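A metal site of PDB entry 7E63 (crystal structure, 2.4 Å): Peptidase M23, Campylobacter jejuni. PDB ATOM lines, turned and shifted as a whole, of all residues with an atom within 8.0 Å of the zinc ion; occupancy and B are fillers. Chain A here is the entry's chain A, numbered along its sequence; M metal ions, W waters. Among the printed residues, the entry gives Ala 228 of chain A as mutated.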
ATOM      1  N   THR A 132       3.620 -14.913 -12.884  1.00  0.00           N
ATOM      2  CA  THR A 132       2.267 -15.451 -12.773  1.00  0.00           C
ATOM      3  C   THR A 132       2.244 -16.797 -12.068  1.00  0.00           C
ATOM      4  O   THR A 132       1.179 -17.295 -11.793  1.00  0.00           O
ATOM      5  CB  THR A 132       1.626 -15.659 -14.127  1.00  0.00           C
ATOM      6  OG1 THR A 132       2.368 -16.661 -14.825  1.00  0.00           O
ATOM      7  CG2 THR A 132       1.692 -14.413 -14.927  1.00  0.00           C
ATOM      8  N   SER A 133       3.403 -17.407 -11.788  1.00  0.00           N
ATOM      9  CA  SER A 133       3.443 -18.635 -10.985  1.00  0.00           C
ATOM     10  C   SER A 133       4.831 -18.904 -10.419  1.00  0.00           C
ATOM     11  O   SER A 133       5.793 -19.177 -11.150  1.00  0.00           O
ATOM     12  CB  SER A 133       3.012 -19.859 -11.761  1.00  0.00           C
ATOM     13  OG  SER A 133       3.088 -21.001 -10.894  1.00  0.00           O
ATOM     14  N   ASP A 134       4.905 -18.862  -9.103  1.00  0.00           N
ATOM     15  CA  ASP A 134       6.170 -18.799  -8.421  1.00  0.00           C
ATOM     16  C   ASP A 134       6.859 -20.132  -8.405  1.00  0.00           C
ATOM     17  O   ASP A 134       6.261 -21.170  -8.666  1.00  0.00           O
ATOM     18  CB  ASP A 134       5.963 -18.341  -6.979  1.00  0.00           C
ATOM     19  CG  ASP A 134       5.888 -16.836  -6.861  1.00  0.00           C
ATOM     20  OD1 ASP A 134       6.959 -16.177  -6.996  1.00  0.00           O
ATOM     21  OD2 ASP A 134       4.766 -16.319  -6.624  1.00  0.00           O
ATOM     22  N   PHE A 135       8.137 -20.083  -8.087  1.00  0.00           N
ATOM     23  CA  PHE A 135       8.922 -21.266  -7.781  1.00  0.00           C
ATOM     24  C   PHE A 135       8.453 -21.925  -6.484  1.00  0.00           C
ATOM     25  O   PHE A 135       8.174 -21.261  -5.507  1.00  0.00           O
ATOM     26  CB  PHE A 135      10.397 -20.876  -7.648  1.00  0.00           C
ATOM     27  CG  PHE A 135      11.295 -22.018  -7.311  1.00  0.00           C
ATOM     28  CD1 PHE A 135      11.793 -22.847  -8.315  1.00  0.00           C
ATOM     29  CD2 PHE A 135      11.629 -22.276  -5.997  1.00  0.00           C
ATOM     30  CE1 PHE A 135      12.609 -23.916  -8.012  1.00  0.00           C
ATOM     31  CE2 PHE A 135      12.463 -23.332  -5.687  1.00  0.00           C
ATOM     32  CZ  PHE A 135      12.958 -24.148  -6.694  1.00  0.00           C
ATOM     33  N   TYR A 148       6.857 -30.482  -7.758  1.00  0.00           N
ATOM     34  CA  TYR A 148       6.814 -29.073  -7.457  1.00  0.00           C
ATOM     35  C   TYR A 148       7.164 -28.343  -8.734  1.00  0.00           C
ATOM     36  O   TYR A 148       7.664 -28.961  -9.673  1.00  0.00           O
ATOM     37  CB  TYR A 148       7.790 -28.726  -6.322  1.00  0.00           C
ATOM     38  CG  TYR A 148       9.239 -28.849  -6.736  1.00  0.00           C
ATOM     39  CD1 TYR A 148       9.849 -30.106  -6.889  1.00  0.00           C
ATOM     40  CD2 TYR A 148      10.002 -27.712  -6.991  1.00  0.00           C
ATOM     41  CE1 TYR A 148      11.170 -30.210  -7.281  1.00  0.00           C
ATOM     42  CE2 TYR A 148      11.322 -27.816  -7.383  1.00  0.00           C
ATOM     43  CZ  TYR A 148      11.890 -29.057  -7.529  1.00  0.00           C
ATOM     44  OH  TYR A 148      13.205 -29.134  -7.927  1.00  0.00           O
ATOM     45  N   HIS A 149       6.887 -27.041  -8.790  1.00  0.00           N
ATOM     46  CA  HIS A 149       7.288 -26.181  -9.902  1.00  0.00           C
ATOM     47  C   HIS A 149       8.754 -25.813  -9.766  1.00  0.00           C
ATOM     48  O   HIS A 149       9.137 -25.100  -8.833  1.00  0.00           O
ATOM     49  CB  HIS A 149       6.453 -24.919  -9.891  1.00  0.00           C
ATOM     50  CG  HIS A 149       6.557 -24.100 -11.128  1.00  0.00           C
ATOM     51  ND1 HIS A 149       6.462 -22.729 -11.115  1.00  0.00           N
ATOM     52  CD2 HIS A 149       6.682 -24.447 -12.426  1.00  0.00           C
ATOM     53  CE1 HIS A 149       6.553 -22.264 -12.352  1.00  0.00           C
ATOM     54  NE2 HIS A 149       6.670 -23.298 -13.169  1.00  0.00           N
ATOM     55  N   SER A 150       9.577 -26.307 -10.699  1.00  0.00           N
ATOM     56  CA  SER A 150      11.042 -26.194 -10.626  1.00  0.00           C
ATOM     57  C   SER A 150      11.679 -24.913 -11.209  1.00  0.00           C
ATOM     58  O   SER A 150      12.907 -24.866 -11.358  1.00  0.00           O
ATOM     59  CB  SER A 150      11.665 -27.405 -11.315  1.00  0.00           C
ATOM     60  OG  SER A 150      11.424 -27.382 -12.708  1.00  0.00           O
ATOM     61  N   GLY A 151      10.872 -23.898 -11.531  1.00  0.00           N
ATOM     62  CA  GLY A 151      11.328 -22.583 -12.016  1.00  0.00           C
ATOM     63  C   GLY A 151      10.236 -21.540 -11.776  1.00  0.00           C
ATOM     64  O   GLY A 151       9.355 -21.741 -10.930  1.00  0.00           O
ATOM     65  N   THR A 152      10.296 -20.430 -12.487  1.00  0.00           N
ATOM     66  CA  THR A 152       9.315 -19.361 -12.326  1.00  0.00           C
ATOM     67  C   THR A 152       8.756 -18.974 -13.667  1.00  0.00           C
ATOM     68  O   THR A 152       9.488 -18.843 -14.659  1.00  0.00           O
ATOM     69  CB  THR A 152       9.945 -18.091 -11.712  1.00  0.00           C
ATOM     70  OG1 THR A 152      10.674 -18.474 -10.562  1.00  0.00           O
ATOM     71  CG2 THR A 152       8.896 -17.125 -11.278  1.00  0.00           C
ATOM     72  N   ASP A 153       7.452 -18.744 -13.711  1.00  0.00           N
ATOM     73  CA  ASP A 153       6.819 -18.371 -14.955  1.00  0.00           C
ATOM     74  C   ASP A 153       6.446 -16.907 -14.961  1.00  0.00           C
ATOM     75  O   ASP A 153       5.885 -16.369 -14.001  1.00  0.00           O
ATOM     76  CB  ASP A 153       5.599 -19.221 -15.261  1.00  0.00           C
ATOM     77  CG  ASP A 153       5.873 -20.705 -15.162  1.00  0.00           C
ATOM     78  OD1 ASP A 153       6.959 -21.206 -15.575  1.00  0.00           O
ATOM     79  OD2 ASP A 153       4.953 -21.388 -14.668  1.00  0.00           O
ATOM     80  N   PHE A 154       6.770 -16.291 -16.093  1.00  0.00           N
ATOM     81  CA  PHE A 154       6.472 -14.925 -16.390  1.00  0.00           C
ATOM     82  C   PHE A 154       5.358 -14.901 -17.423  1.00  0.00           C
ATOM     83  O   PHE A 154       5.341 -15.690 -18.360  1.00  0.00           O
ATOM     84  CB  PHE A 154       7.677 -14.272 -17.029  1.00  0.00           C
ATOM     85  CG  PHE A 154       8.861 -14.135 -16.130  1.00  0.00           C
ATOM     86  CD1 PHE A 154       9.612 -15.238 -15.762  1.00  0.00           C
ATOM     87  CD2 PHE A 154       9.254 -12.856 -15.662  1.00  0.00           C
ATOM     88  CE1 PHE A 154      10.715 -15.103 -14.943  1.00  0.00           C
ATOM     89  CE2 PHE A 154      10.361 -12.714 -14.850  1.00  0.00           C
ATOM     90  CZ  PHE A 154      11.097 -13.843 -14.485  1.00  0.00           C
ATOM     91  N   TYR A 196      11.998 -22.461 -21.017  1.00  0.00           N
ATOM     92  CA  TYR A 196      11.083 -23.471 -21.513  1.00  0.00           C
ATOM     93  C   TYR A 196       9.762 -22.901 -22.131  1.00  0.00           C
ATOM     94  O   TYR A 196       9.441 -21.727 -21.988  1.00  0.00           O
ATOM     95  CB  TYR A 196      10.751 -24.444 -20.398  1.00  0.00           C
ATOM     96  CG  TYR A 196      11.912 -25.197 -19.784  1.00  0.00           C
ATOM     97  CD1 TYR A 196      13.195 -25.198 -20.355  1.00  0.00           C
ATOM     98  CD2 TYR A 196      11.712 -25.965 -18.645  1.00  0.00           C
ATOM     99  CE1 TYR A 196      14.237 -25.921 -19.779  1.00  0.00           C
ATOM    100  CE2 TYR A 196      12.735 -26.677 -18.069  1.00  0.00           C
ATOM    101  CZ  TYR A 196      13.998 -26.667 -18.640  1.00  0.00           C
ATOM    102  OH  TYR A 196      14.996 -27.415 -18.038  1.00  0.00           O
ATOM    103  N   HIS A 197       9.059 -23.781 -22.849  1.00  0.00           N
ATOM    104  CA  HIS A 197       7.754 -23.551 -23.500  1.00  0.00           C
ATOM    105  C   HIS A 197       7.752 -22.572 -24.617  1.00  0.00           C
ATOM    106  O   HIS A 197       6.716 -22.025 -24.952  1.00  0.00           O
ATOM    107  CB  HIS A 197       6.711 -23.173 -22.475  1.00  0.00           C
ATOM    108  CG  HIS A 197       6.800 -23.966 -21.208  1.00  0.00           C
ATOM    109  ND1 HIS A 197       6.952 -25.329 -21.194  1.00  0.00           N
ATOM    110  CD2 HIS A 197       6.734 -23.580 -19.912  1.00  0.00           C
ATOM    111  CE1 HIS A 197       6.970 -25.758 -19.949  1.00  0.00           C
ATOM    112  NE2 HIS A 197       6.837 -24.716 -19.148  1.00  0.00           N
ATOM    113  N   ARG A 223       4.568 -29.253 -21.670  1.00  0.00           N
ATOM    114  CA  ARG A 223       3.655 -29.450 -20.557  1.00  0.00           C
ATOM    115  C   ARG A 223       3.432 -28.163 -19.773  1.00  0.00           C
ATOM    116  O   ARG A 223       4.142 -27.881 -18.831  1.00  0.00           O
ATOM    117  CB  ARG A 223       4.204 -30.523 -19.623  1.00  0.00           C
ATOM    118  CG  ARG A 223       3.149 -31.078 -18.670  1.00  0.00           C
ATOM    119  CD  ARG A 223       3.470 -32.508 -18.239  1.00  0.00           C
ATOM    120  NE  ARG A 223       2.397 -33.102 -17.431  1.00  0.00           N
ATOM    121  CZ  ARG A 223       2.111 -32.762 -16.173  1.00  0.00           C
ATOM    122  NH1 ARG A 223       1.107 -33.365 -15.535  1.00  0.00           N
ATOM    123  NH2 ARG A 223       2.804 -31.835 -15.535  1.00  0.00           N
ATOM    124  N   VAL A 224       2.441 -27.396 -20.181  1.00  0.00           N
ATOM    125  CA  VAL A 224       2.163 -26.106 -19.580  1.00  0.00           C
ATOM    126  C   VAL A 224       0.712 -25.802 -19.961  1.00  0.00           C
ATOM    127  O   VAL A 224       0.203 -26.348 -20.934  1.00  0.00           O
ATOM    128  CB  VAL A 224       3.151 -25.025 -20.089  1.00  0.00           C
ATOM    129  CG1 VAL A 224       2.999 -24.767 -21.590  1.00  0.00           C
ATOM    130  CG2 VAL A 224       2.973 -23.713 -19.361  1.00  0.00           C
ATOM    131  N   ALA A 228       3.347 -18.755 -21.760  1.00  0.00           N
ATOM    132  CA  ALA A 228       4.086 -18.265 -20.616  1.00  0.00           C
ATOM    133  C   ALA A 228       5.564 -18.511 -20.908  1.00  0.00           C
ATOM    134  O   ALA A 228       5.891 -19.420 -21.691  1.00  0.00           O
ATOM    135  CB  ALA A 228       3.682 -18.988 -19.332  1.00  0.00           C
ATOM    136  N   LEU A 229       6.451 -17.731 -20.293  1.00  0.00           N
ATOM    137  CA  LEU A 229       7.849 -18.091 -20.252  1.00  0.00           C
ATOM    138  C   LEU A 229       8.195 -18.665 -18.887  1.00  0.00           C
ATOM    139  O   LEU A 229       8.015 -17.976 -17.873  1.00  0.00           O
ATOM    140  CB  LEU A 229       8.768 -16.918 -20.503  1.00  0.00           C
ATOM    141  CG  LEU A 229      10.220 -17.357 -20.248  1.00  0.00           C
ATOM    142  CD1 LEU A 229      10.777 -18.085 -21.455  1.00  0.00           C
ATOM    143  CD2 LEU A 229      11.088 -16.202 -19.863  1.00  0.00           C
ATOM    144  N   HIS A 230       8.755 -19.891 -18.883  1.00  0.00           N
ATOM    145  CA  HIS A 230       9.230 -20.565 -17.686  1.00  0.00           C
ATOM    146  C   HIS A 230      10.730 -20.375 -17.620  1.00  0.00           C
ATOM    147  O   HIS A 230      11.416 -20.667 -18.594  1.00  0.00           O
ATOM    148  CB  HIS A 230       8.905 -22.055 -17.742  1.00  0.00           C
ATOM    149  CG  HIS A 230       9.638 -22.891 -16.732  1.00  0.00           C
ATOM    150  ND1 HIS A 230       9.049 -23.384 -15.599  1.00  0.00           N
ATOM    151  CD2 HIS A 230      10.915 -23.358 -16.718  1.00  0.00           C
ATOM    152  CE1 HIS A 230       9.922 -24.100 -14.912  1.00  0.00           C
ATOM    153  NE2 HIS A 230      11.064 -24.108 -15.573  1.00  0.00           N
ATOM    154  N   PHE A 231      11.216 -19.884 -16.469  1.00  0.00           N
ATOM    155  CA  PHE A 231      12.634 -19.540 -16.260  1.00  0.00           C
ATOM    156  C   PHE A 231      13.137 -20.332 -15.091  1.00  0.00           C
ATOM    157  O   PHE A 231      12.543 -20.268 -14.019  1.00  0.00           O
ATOM    158  CB  PHE A 231      12.790 -18.047 -15.973  1.00  0.00           C
ATOM    159  CG  PHE A 231      14.225 -17.604 -15.761  1.00  0.00           C
ATOM    160  CD1 PHE A 231      15.180 -17.773 -16.761  1.00  0.00           C
ATOM    161  CD2 PHE A 231      14.624 -17.015 -14.559  1.00  0.00           C
ATOM    162  CE1 PHE A 231      16.507 -17.354 -16.576  1.00  0.00           C
ATOM    163  CE2 PHE A 231      15.934 -16.599 -14.370  1.00  0.00           C
ATOM    164  CZ  PHE A 231      16.887 -16.754 -15.373  1.00  0.00           C
ATOM    165  N   GLY A 232      14.198 -21.114 -15.282  1.00  0.00           N
ATOM    166  CA  GLY A 232      14.741 -21.896 -14.203  1.00  0.00           C
ATOM    167  C   GLY A 232      16.240 -21.695 -14.050  1.00  0.00           C
ATOM    168  O   GLY A 232      16.898 -21.182 -14.936  1.00  0.00           O
HETATM  169 ZN    ZN M   1       6.994 -23.058 -14.956  1.00  0.00          ZN
HETATM  170  O   HOH W   1       6.274 -24.714 -16.084  1.00  0.00           O
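O of Gly 151 is in hydrogen-bond range of ND1 of His 149, 3.1 Å away.
The backbone carbonyl oxygen of Asp 153 sits at hydrogen-bond distance from the backbone NH of Thr 132 (2.9 Å).
A ring nitrogen (ND1) of His 149 sits at hydrogen-bond distance from the backbone carbonyl oxygen of Asp 134, at 2.9 Å.
The backbone carbonyl oxygen of His 230 sits at hydrogen-bond distance from the backbone NH of Tyr 196, at 3.1 Å.
The backbone NH (N) of Asp 153 is in hydrogen-bond range of the backbone carbonyl oxygen (O) of Ser 133, 3.1 Å away.
Of the 20 residues printed, 3 come within 4 Å of the zinc ion.
The nearest printed residue that does not touch the zinc ion is His 197 (4.5 Å).
The zinc ion is bound by a ring nitrogen (NE2) of His 149 (1.8 Å), the side-chain carboxylate of Asp 153 (2.0 Å), water W1 (2.1 Å) and a ring nitrogen (ND1) of His 230 (2.2 Å).
Slightly farther from the zinc ion lies OD2 of Asp 153 (2.7 Å).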
